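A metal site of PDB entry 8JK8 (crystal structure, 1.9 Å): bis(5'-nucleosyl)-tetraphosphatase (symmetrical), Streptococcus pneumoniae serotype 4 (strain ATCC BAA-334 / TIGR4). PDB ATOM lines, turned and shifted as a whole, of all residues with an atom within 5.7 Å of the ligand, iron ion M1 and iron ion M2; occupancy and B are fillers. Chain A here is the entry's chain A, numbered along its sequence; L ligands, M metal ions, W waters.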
ATOM      1  N   ARG A  26      -4.591   6.295  -8.538  1.00  0.00           N
ATOM      2  CA  ARG A  26      -5.125   5.053  -7.994  1.00  0.00           C
ATOM      3  C   ARG A  26      -6.634   5.158  -7.720  1.00  0.00           C
ATOM      4  O   ARG A  26      -7.364   4.192  -7.967  1.00  0.00           O
ATOM      5  CB  ARG A  26      -4.328   4.612  -6.763  1.00  0.00           C
ATOM      6  CG  ARG A  26      -4.723   3.275  -6.152  1.00  0.00           C
ATOM      7  CD  ARG A  26      -4.605   2.126  -7.145  1.00  0.00           C
ATOM      8  NE  ARG A  26      -3.223   1.982  -7.567  1.00  0.00           N
ATOM      9  CZ  ARG A  26      -2.779   1.165  -8.512  1.00  0.00           C
ATOM     10  NH1 ARG A  26      -1.491   1.127  -8.783  1.00  0.00           N
ATOM     11  NH2 ARG A  26      -3.625   0.381  -9.178  1.00  0.00           N
ATOM     12  N   HIS A  29      -8.392   5.062 -10.999  1.00  0.00           N
ATOM     13  CA  HIS A  29      -8.363   3.641 -11.385  1.00  0.00           C
ATOM     14  C   HIS A  29      -9.550   2.892 -10.753  1.00  0.00           C
ATOM     15  O   HIS A  29     -10.284   2.201 -11.454  1.00  0.00           O
ATOM     16  CB  HIS A  29      -7.022   2.976 -11.021  1.00  0.00           C
ATOM     17  CG  HIS A  29      -7.040   1.466 -11.049  1.00  0.00           C
ATOM     18  ND1 HIS A  29      -7.250   0.746 -12.218  1.00  0.00           N
ATOM     19  CD2 HIS A  29      -6.884   0.538 -10.075  1.00  0.00           C
ATOM     20  CE1 HIS A  29      -7.209  -0.542 -11.956  1.00  0.00           C
ATOM     21  NE2 HIS A  29      -6.991  -0.693 -10.662  1.00  0.00           N
ATOM     22  N   VAL A  33     -12.639   1.010 -12.517  1.00  0.00           N
ATOM     23  CA  VAL A  33     -12.987  -0.389 -12.262  1.00  0.00           C
ATOM     24  C   VAL A  33     -14.433  -0.550 -11.793  1.00  0.00           C
ATOM     25  O   VAL A  33     -15.100  -1.486 -12.189  1.00  0.00           O
ATOM     26  CB  VAL A  33     -12.002  -1.063 -11.273  1.00  0.00           C
ATOM     27  CG1 VAL A  33     -12.412  -2.504 -10.991  1.00  0.00           C
ATOM     28  CG2 VAL A  33     -10.597  -1.081 -11.864  1.00  0.00           C
ATOM     29  N   HIS A  58     -11.569  -2.636  -4.771  1.00  0.00           N
ATOM     30  CA  HIS A  58     -10.586  -3.715  -4.955  1.00  0.00           C
ATOM     31  C   HIS A  58      -9.147  -3.290  -4.555  1.00  0.00           C
ATOM     32  O   HIS A  58      -8.394  -4.101  -3.992  1.00  0.00           O
ATOM     33  CB  HIS A  58     -10.649  -4.276  -6.383  1.00  0.00           C
ATOM     34  CG  HIS A  58      -9.909  -3.445  -7.375  1.00  0.00           C
ATOM     35  ND1 HIS A  58     -10.365  -2.221  -7.799  1.00  0.00           N
ATOM     36  CD2 HIS A  58      -8.719  -3.653  -7.988  1.00  0.00           C
ATOM     37  CE1 HIS A  58      -9.482  -1.697  -8.638  1.00  0.00           C
ATOM     38  NE2 HIS A  58      -8.475  -2.531  -8.759  1.00  0.00           N
ATOM     39  N   ASP A  59      -8.785  -2.030  -4.820  1.00  0.00           N
ATOM     40  CA  ASP A  59      -7.443  -1.495  -4.563  1.00  0.00           C
ATOM     41  C   ASP A  59      -7.398  -0.549  -3.370  1.00  0.00           C
ATOM     42  O   ASP A  59      -6.454   0.230  -3.219  1.00  0.00           O
ATOM     43  CB  ASP A  59      -6.843  -0.818  -5.809  1.00  0.00           C
ATOM     44  CG  ASP A  59      -6.112  -1.793  -6.725  1.00  0.00           C
ATOM     45  OD1 ASP A  59      -5.868  -2.944  -6.343  1.00  0.00           O
ATOM     46  OD2 ASP A  59      -5.844  -1.418  -7.868  1.00  0.00           O
ATOM     47  N   LYS A  62      -4.170  -0.630  -1.416  1.00  0.00           N
ATOM     48  CA  LYS A  62      -2.971  -0.592  -2.281  1.00  0.00           C
ATOM     49  C   LYS A  62      -1.775   0.128  -1.636  1.00  0.00           C
ATOM     50  O   LYS A  62      -0.629  -0.235  -1.901  1.00  0.00           O
ATOM     51  CB  LYS A  62      -3.296   0.012  -3.658  1.00  0.00           C
ATOM     52  CG  LYS A  62      -2.193  -0.060  -4.716  1.00  0.00           C
ATOM     53  CD  LYS A  62      -1.906  -1.480  -5.209  1.00  0.00           C
ATOM     54  CE  LYS A  62      -0.732  -1.493  -6.173  1.00  0.00           C
ATOM     55  NZ  LYS A  62      -0.718  -2.664  -7.100  1.00  0.00           N
ATOM     56  N   TRP A  85       6.083 -12.912   0.529  1.00  0.00           N
ATOM     57  CA  TRP A  85       5.605 -12.170  -0.628  1.00  0.00           C
ATOM     58  C   TRP A  85       5.596 -10.691  -0.283  1.00  0.00           C
ATOM     59  O   TRP A  85       6.309 -10.276   0.631  1.00  0.00           O
ATOM     60  CB  TRP A  85       4.250 -12.738  -1.043  1.00  0.00           C
ATOM     61  CG  TRP A  85       4.448 -14.179  -1.400  1.00  0.00           C
ATOM     62  CD1 TRP A  85       4.313 -15.254  -0.570  1.00  0.00           C
ATOM     63  CD2 TRP A  85       4.874 -14.692  -2.653  1.00  0.00           C
ATOM     64  NE1 TRP A  85       4.620 -16.407  -1.243  1.00  0.00           N
ATOM     65  CE2 TRP A  85       4.962 -16.100  -2.530  1.00  0.00           C
ATOM     66  CE3 TRP A  85       5.177 -14.103  -3.897  1.00  0.00           C
ATOM     67  CZ2 TRP A  85       5.327 -16.930  -3.589  1.00  0.00           C
ATOM     68  CZ3 TRP A  85       5.536 -14.931  -4.944  1.00  0.00           C
ATOM     69  CH2 TRP A  85       5.626 -16.324  -4.782  1.00  0.00           C
ATOM     70  N   ASN A  88       1.875  -6.655  -3.935  1.00  0.00           N
ATOM     71  CA  ASN A  88       1.168  -7.272  -5.064  1.00  0.00           C
ATOM     72  C   ASN A  88       0.192  -8.375  -4.666  1.00  0.00           C
ATOM     73  O   ASN A  88      -0.965  -8.321  -5.064  1.00  0.00           O
ATOM     74  CB  ASN A  88       2.159  -7.779  -6.098  1.00  0.00           C
ATOM     75  CG  ASN A  88       2.862  -6.646  -6.836  1.00  0.00           C
ATOM     76  OD1 ASN A  88       2.434  -5.489  -6.783  1.00  0.00           O
ATOM     77  ND2 ASN A  88       3.930  -6.990  -7.553  1.00  0.00           N
ATOM     78  N   VAL A  89       0.679  -9.336  -3.878  1.00  0.00           N
ATOM     79  CA  VAL A  89      -0.145 -10.403  -3.312  1.00  0.00           C
ATOM     80  C   VAL A  89      -1.005  -9.878  -2.156  1.00  0.00           C
ATOM     81  O   VAL A  89      -2.172 -10.256  -2.016  1.00  0.00           O
ATOM     82  CB  VAL A  89       0.711 -11.624  -2.842  1.00  0.00           C
ATOM     83  CG1 VAL A  89      -0.130 -12.668  -2.122  1.00  0.00           C
ATOM     84  CG2 VAL A  89       1.397 -12.289  -4.032  1.00  0.00           C
ATOM     85  N   HIS A  91      -2.252  -6.784  -1.089  1.00  0.00           N
ATOM     86  CA  HIS A  91      -3.262  -5.713  -1.114  1.00  0.00           C
ATOM     87  C   HIS A  91      -4.699  -6.267  -1.300  1.00  0.00           C
ATOM     88  O   HIS A  91      -5.628  -5.787  -0.668  1.00  0.00           O
ATOM     89  CB  HIS A  91      -2.857  -4.552  -2.061  1.00  0.00           C
ATOM     90  CG  HIS A  91      -3.084  -4.818  -3.516  1.00  0.00           C
ATOM     91  ND1 HIS A  91      -2.127  -5.417  -4.320  1.00  0.00           N
ATOM     92  CD2 HIS A  91      -4.124  -4.523  -4.329  1.00  0.00           C
ATOM     93  CE1 HIS A  91      -2.599  -5.508  -5.557  1.00  0.00           C
ATOM     94  NE2 HIS A  91      -3.806  -4.983  -5.579  1.00  0.00           N
ATOM     95  N   HIS A 117      -8.505 -10.675  -6.579  1.00  0.00           N
ATOM     96  CA  HIS A 117      -8.488  -9.815  -7.792  1.00  0.00           C
ATOM     97  C   HIS A 117      -7.144  -9.806  -8.551  1.00  0.00           C
ATOM     98  O   HIS A 117      -7.127  -9.559  -9.759  1.00  0.00           O
ATOM     99  CB  HIS A 117      -8.986  -8.369  -7.505  1.00  0.00           C
ATOM    100  CG  HIS A 117      -7.914  -7.445  -6.995  1.00  0.00           C
ATOM    101  ND1 HIS A 117      -7.736  -7.196  -5.647  1.00  0.00           N
ATOM    102  CD2 HIS A 117      -6.984  -6.692  -7.645  1.00  0.00           C
ATOM    103  CE1 HIS A 117      -6.726  -6.355  -5.491  1.00  0.00           C
ATOM    104  NE2 HIS A 117      -6.254  -6.027  -6.680  1.00  0.00           N
ATOM    105  N   THR A 118      -6.045 -10.052  -7.837  1.00  0.00           N
ATOM    106  CA  THR A 118      -4.664 -10.000  -8.397  1.00  0.00           C
ATOM    107  C   THR A 118      -4.234 -11.376  -8.925  1.00  0.00           C
ATOM    108  O   THR A 118      -3.737 -11.489 -10.049  1.00  0.00           O
ATOM    109  CB  THR A 118      -3.613  -9.496  -7.355  1.00  0.00           C
ATOM    110  OG1 THR A 118      -4.017  -8.241  -6.793  1.00  0.00           O
ATOM    111  CG2 THR A 118      -2.224  -9.329  -7.994  1.00  0.00           C
ATOM    112  N   VAL A 119      -4.447 -12.400  -8.109  1.00  0.00           N
ATOM    113  CA  VAL A 119      -3.932 -13.762  -8.339  1.00  0.00           C
ATOM    114  C   VAL A 119      -4.945 -14.766  -8.903  1.00  0.00           C
ATOM    115  O   VAL A 119      -4.556 -15.834  -9.394  1.00  0.00           O
ATOM    116  CB  VAL A 119      -3.327 -14.360  -7.044  1.00  0.00           C
ATOM    117  CG1 VAL A 119      -2.143 -13.518  -6.585  1.00  0.00           C
ATOM    118  CG2 VAL A 119      -4.378 -14.498  -5.933  1.00  0.00           C
ATOM    119  N   ASP A 135     -10.566  -4.844 -13.674  1.00  0.00           N
ATOM    120  CA  ASP A 135      -9.321  -4.235 -13.200  1.00  0.00           C
ATOM    121  C   ASP A 135      -8.366  -3.952 -14.390  1.00  0.00           C
ATOM    122  O   ASP A 135      -7.717  -2.880 -14.493  1.00  0.00           O
ATOM    123  CB  ASP A 135      -8.691  -5.199 -12.186  1.00  0.00           C
ATOM    124  CG  ASP A 135      -7.453  -4.640 -11.532  1.00  0.00           C
ATOM    125  OD1 ASP A 135      -7.347  -3.397 -11.415  1.00  0.00           O
ATOM    126  OD2 ASP A 135      -6.582  -5.447 -11.160  1.00  0.00           O
ATOM    127  N   ARG A 141      -6.881   2.532 -18.433  1.00  0.00           N
ATOM    128  CA  ARG A 141      -5.725   1.711 -18.819  1.00  0.00           C
ATOM    129  C   ARG A 141      -5.407   1.907 -20.287  1.00  0.00           C
ATOM    130  O   ARG A 141      -6.312   2.050 -21.105  1.00  0.00           O
ATOM    131  CB  ARG A 141      -5.963   0.220 -18.582  1.00  0.00           C
ATOM    132  CG  ARG A 141      -6.451  -0.193 -17.204  1.00  0.00           C
ATOM    133  CD  ARG A 141      -5.393  -0.191 -16.109  1.00  0.00           C
ATOM    134  NE  ARG A 141      -4.199  -0.966 -16.421  1.00  0.00           N
ATOM    135  CZ  ARG A 141      -3.903  -2.123 -15.832  1.00  0.00           C
ATOM    136  NH1 ARG A 141      -2.775  -2.737 -16.149  1.00  0.00           N
ATOM    137  NH2 ARG A 141      -4.715  -2.658 -14.926  1.00  0.00           N
ATOM    138  N   GLU A 164      -5.781 -12.366 -19.749  1.00  0.00           N
ATOM    139  CA  GLU A 164      -5.129 -11.573 -18.701  1.00  0.00           C
ATOM    140  C   GLU A 164      -4.114 -12.407 -17.900  1.00  0.00           C
ATOM    141  O   GLU A 164      -2.964 -11.967 -17.702  1.00  0.00           O
ATOM    142  CB  GLU A 164      -6.149 -10.943 -17.766  1.00  0.00           C
ATOM    143  CG  GLU A 164      -5.498 -10.212 -16.597  1.00  0.00           C
ATOM    144  CD  GLU A 164      -6.466  -9.594 -15.627  1.00  0.00           C
ATOM    145  OE1 GLU A 164      -7.694  -9.571 -15.879  1.00  0.00           O
ATOM    146  OE2 GLU A 164      -5.963  -9.074 -14.601  1.00  0.00           O
ATOM    147  N   THR A 168      -0.016 -11.917 -17.686  1.00  0.00           N
ATOM    148  CA  THR A 168       0.591 -11.674 -16.380  1.00  0.00           C
ATOM    149  C   THR A 168       1.736 -12.646 -16.119  1.00  0.00           C
ATOM    150  O   THR A 168       2.832 -12.225 -15.745  1.00  0.00           O
ATOM    151  CB  THR A 168      -0.487 -11.757 -15.276  1.00  0.00           C
ATOM    152  OG1 THR A 168      -1.378 -10.653 -15.456  1.00  0.00           O
ATOM    153  CG2 THR A 168       0.114 -11.704 -13.868  1.00  0.00           C
ATOM    154  N   TYR A 171       4.684 -11.878 -18.543  1.00  0.00           N
ATOM    155  CA  TYR A 171       5.397 -10.666 -18.118  1.00  0.00           C
ATOM    156  C   TYR A 171       6.225 -10.877 -16.833  1.00  0.00           C
ATOM    157  O   TYR A 171       7.353 -10.402 -16.771  1.00  0.00           O
ATOM    158  CB  TYR A 171       4.428  -9.481 -17.953  1.00  0.00           C
ATOM    159  CG  TYR A 171       5.020  -8.243 -17.289  1.00  0.00           C
ATOM    160  CD1 TYR A 171       5.711  -7.279 -18.042  1.00  0.00           C
ATOM    161  CD2 TYR A 171       4.859  -8.016 -15.916  1.00  0.00           C
ATOM    162  CE1 TYR A 171       6.237  -6.138 -17.448  1.00  0.00           C
ATOM    163  CE2 TYR A 171       5.389  -6.885 -15.302  1.00  0.00           C
ATOM    164  CZ  TYR A 171       6.068  -5.940 -16.073  1.00  0.00           C
ATOM    165  OH  TYR A 171       6.584  -4.822 -15.448  1.00  0.00           O
ATOM    166  N   LEU A 172       5.661 -11.574 -15.836  1.00  0.00           N
ATOM    167  CA  LEU A 172       6.423 -11.869 -14.624  1.00  0.00           C
ATOM    168  C   LEU A 172       7.686 -12.682 -14.928  1.00  0.00           C
ATOM    169  O   LEU A 172       8.762 -12.381 -14.393  1.00  0.00           O
ATOM    170  CB  LEU A 172       5.562 -12.562 -13.555  1.00  0.00           C
ATOM    171  CG  LEU A 172       4.455 -11.707 -12.946  1.00  0.00           C
ATOM    172  CD1 LEU A 172       3.522 -12.588 -12.147  1.00  0.00           C
ATOM    173  CD2 LEU A 172       5.001 -10.565 -12.073  1.00  0.00           C
ATOM    174  N   PRO A 178       9.156 -13.423  -8.969  1.00  0.00           N
ATOM    175  CA  PRO A 178       8.474 -14.623  -8.455  1.00  0.00           C
ATOM    176  C   PRO A 178       6.983 -14.626  -8.827  1.00  0.00           C
ATOM    177  O   PRO A 178       6.379 -13.562  -8.968  1.00  0.00           O
ATOM    178  CB  PRO A 178       8.617 -14.494  -6.937  1.00  0.00           C
ATOM    179  CG  PRO A 178       9.740 -13.542  -6.700  1.00  0.00           C
ATOM    180  CD  PRO A 178       9.772 -12.627  -7.891  1.00  0.00           C
ATOM    181  N   ILE A 179       6.435 -15.813  -9.036  1.00  0.00           N
ATOM    182  CA  ILE A 179       5.030 -15.967  -9.428  1.00  0.00           C
ATOM    183  C   ILE A 179       4.283 -16.678  -8.310  1.00  0.00           C
ATOM    184  O   ILE A 179       4.602 -17.834  -7.972  1.00  0.00           O
ATOM    185  CB  ILE A 179       4.895 -16.733 -10.775  1.00  0.00           C
ATOM    186  CG1 ILE A 179       5.475 -15.893 -11.932  1.00  0.00           C
ATOM    187  CG2 ILE A 179       3.443 -17.140 -11.050  1.00  0.00           C
ATOM    188  CD1 ILE A 179       5.826 -16.680 -13.196  1.00  0.00           C
ATOM    189  N   TYR A 180       3.294 -16.004  -7.733  1.00  0.00           N
ATOM    190  CA  TYR A 180       2.505 -16.591  -6.664  1.00  0.00           C
ATOM    191  C   TYR A 180       1.869 -17.893  -7.131  1.00  0.00           C
ATOM    192  O   TYR A 180       1.247 -17.910  -8.207  1.00  0.00           O
ATOM    193  CB  TYR A 180       1.441 -15.598  -6.170  1.00  0.00           C
ATOM    194  CG  TYR A 180       0.840 -16.016  -4.860  1.00  0.00           C
ATOM    195  CD1 TYR A 180       1.626 -16.108  -3.719  1.00  0.00           C
ATOM    196  CD2 TYR A 180      -0.523 -16.305  -4.757  1.00  0.00           C
ATOM    197  CE1 TYR A 180       1.085 -16.492  -2.505  1.00  0.00           C
ATOM    198  CE2 TYR A 180      -1.080 -16.675  -3.537  1.00  0.00           C
ATOM    199  CZ  TYR A 180      -0.269 -16.777  -2.423  1.00  0.00           C
ATOM    200  OH  TYR A 180      -0.799 -17.154  -1.213  1.00  0.00           O
ATOM    201  N   THR A 183      -1.528 -17.937  -8.692  1.00  0.00           N
ATOM    202  CA  THR A 183      -1.611 -17.405 -10.068  1.00  0.00           C
ATOM    203  C   THR A 183      -1.494 -18.538 -11.089  1.00  0.00           C
ATOM    204  O   THR A 183      -2.228 -18.532 -12.095  1.00  0.00           O
ATOM    205  CB  THR A 183      -0.596 -16.251 -10.298  1.00  0.00           C
ATOM    206  OG1 THR A 183      -0.892 -15.218  -9.361  1.00  0.00           O
ATOM    207  CG2 THR A 183      -0.656 -15.667 -11.744  1.00  0.00           C
HETATM  208  N1  LIG L   1       1.666  -9.830  -9.606  1.00  0.00           N
HETATM  209  C1  LIG L   1       0.646 -10.691 -10.103  1.00  0.00           C
HETATM  210  N2  LIG L   1       0.680 -12.022  -9.837  1.00  0.00           N
HETATM  211  C2  LIG L   1       1.675 -12.569  -9.111  1.00  0.00           C
HETATM  212  C3  LIG L   1       2.708 -11.762  -8.598  1.00  0.00           C
HETATM  213  C4  LIG L   1       2.676 -10.379  -8.865  1.00  0.00           C
HETATM  214  O1  LIG L   1      -0.309 -10.255 -10.783  1.00  0.00           O
HETATM  215  O2  LIG L   1       1.674 -13.811  -8.893  1.00  0.00           O
HETATM  216  C5  LIG L   1       1.675  -8.357  -9.869  1.00  0.00           C
HETATM  217  C6  LIG L   1       1.252  -7.902 -11.274  1.00  0.00           C
HETATM  218  O3  LIG L   1       2.207  -8.240 -12.284  1.00  0.00           O
HETATM  219  C7  LIG L   1       0.967  -6.405 -11.086  1.00  0.00           C
HETATM  220  C8  LIG L   1       0.660  -6.287  -9.597  1.00  0.00           C
HETATM  221  O4  LIG L   1       0.798  -7.600  -9.023  1.00  0.00           O
HETATM  222  O5  LIG L   1       2.102  -5.575 -11.377  1.00  0.00           O
HETATM  223  C9  LIG L   1      -0.697  -5.680  -9.285  1.00  0.00           C
HETATM  224  O6  LIG L   1      -1.751  -6.457  -9.860  1.00  0.00           O
HETATM  225  P1  LIG L   1      -3.318  -6.047  -9.779  1.00  0.00           P
HETATM  226  O7  LIG L   1      -3.722  -6.116  -8.334  1.00  0.00           O
HETATM  227  O8  LIG L   1      -4.054  -6.979 -10.740  1.00  0.00           O
HETATM  228  O9  LIG L   1      -3.353  -4.533 -10.426  1.00  0.00           O
HETATM  229  P2  LIG L   1      -3.205  -3.026  -9.774  1.00  0.00           P
HETATM  230  O10 LIG L   1      -3.425  -3.121  -8.261  1.00  0.00           O
HETATM  231  O11 LIG L   1      -4.324  -2.261 -10.494  1.00  0.00           O
HETATM  232  O12 LIG L   1      -1.819  -2.535 -10.171  1.00  0.00           O
HETATM  233 FE    FE M   1      -4.921  -4.617  -7.336  1.00  0.00          FE
HETATM  234 FE    FE M   2      -6.525  -2.387  -9.707  1.00  0.00          FE
HETATM  235  O   HOH W   1      -3.839  -0.444 -12.604  1.00  0.00           O
HETATM  236  O   HOH W   2      -6.509  -8.277 -11.839  1.00  0.00           O
HETATM  237  O   HOH W   3      -4.600  -5.273 -13.746  1.00  0.00           O
HETATM  238  O   HOH W   4      -5.889  -4.001  -9.011  1.00  0.00           O
HETATM  239  O   HOH W   5      -2.951  -9.439 -11.598  1.00  0.00           O
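The backbone NH of Tyr 180 sits at hydrogen-bond distance from an oxygen (O2) of the ligand (3.0 Å).
An oxygen (O2) of the ligand sits at hydrogen-bond distance from the side-chain hydroxyl (OG1) of Thr 183 (3.0 Å).
OD1 of Asn 88 sits close to O4 of the ligand, at 3.5 Å.
NH2 of Arg 26 lies within salt-bridge range of O12 of the ligand (3.6 Å).
OG1 of Thr 118 lies close to O7 of the ligand, 2.6 Å away.
NZ of Lys 62 lies within salt-bridge range of O12 of the ligand (3.3 Å).
A ring nitrogen (NE2) of His 117 lies close to the side-chain hydroxyl (OG1) of Thr 118, 3.1 Å away.
O of Asp 135 is in hydrogen-bond range of NH2 of Arg 141 (3.0 Å).
OG1 of Thr 168 is in hydrogen-bond range of O of Glu 164.
The guanidinium group (NH2) of Arg 26 sits close to the side-chain carboxylate (OD2) of Asp 59 (3.1 Å).
The side-chain hydroxyl of Thr 118 lies close to a ring nitrogen (NE2) of His 91 (3.5 Å).
A ring nitrogen (ND1) of His 91 is in hydrogen-bond range of the backbone carbonyl oxygen of Asn 88, 3.2 Å away.
Thr 168 touches the ligand (CG2 to O1, 3.4 Å).
CD1 of Leu 172 touches C2 of the ligand (3.6 Å).
C of Ile 179 touches O2 of the ligand, 3.9 Å away.
Hydrophobic or aromatic side chains within 4 Å of the ligand: His 29, His 91, His 117, Leu 172 and Tyr 180.
Within 4 Å of the ligand: Arg 26, His 29, Asp 59, Lys 62, Asn 88, His 91, His 117, Thr 118, Asp 135, Thr 168, Leu 172, Ile 179, Tyr 180 and Thr 183.
The nearest printed residue that does not touch the ligand is Pro 178 (4.1 Å).
Merely in contact with iron ion M1: Thr 118.
The nearest printed residue that does not touch iron ion M1 is Asp 135 (4.3 Å).
Along chain A the residues within 4 Å of iron ion M2 span positions 29 to 135.
Iron ion M1 is bound by water W4 (2.0 Å), NE2 of His 117 (2.0 Å), NE2 of His 91 (2.1 Å), OD1 of Asp 59 (2.2 Å), O7 of the ligand (2.2 Å) and O10 of the ligand (2.3 Å).
Iron ion M2 is bound by water W4, NE2 of His 29, OD1 of Asp 135, NE2 of His 58, OD2 of Asp 59 and O11 of the ligand.
Water W4 bridges the side-chain carboxylate (OD2) of Asp 135 (2.7 Å) and an oxygen (O9) of the ligand (3.0 Å).
Water W5 lies within hydrogen-bond range of the backbone carbonyl oxygen of Thr 118 (2.7 Å) and an oxygen (O8) of the ligand (2.8 Å).
Water W3 lies within hydrogen-bond range of NH2 of Arg 141 (2.9 Å), OD2 of Asp 135 (3.3 Å) and O8 of the ligand (3.5 Å).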
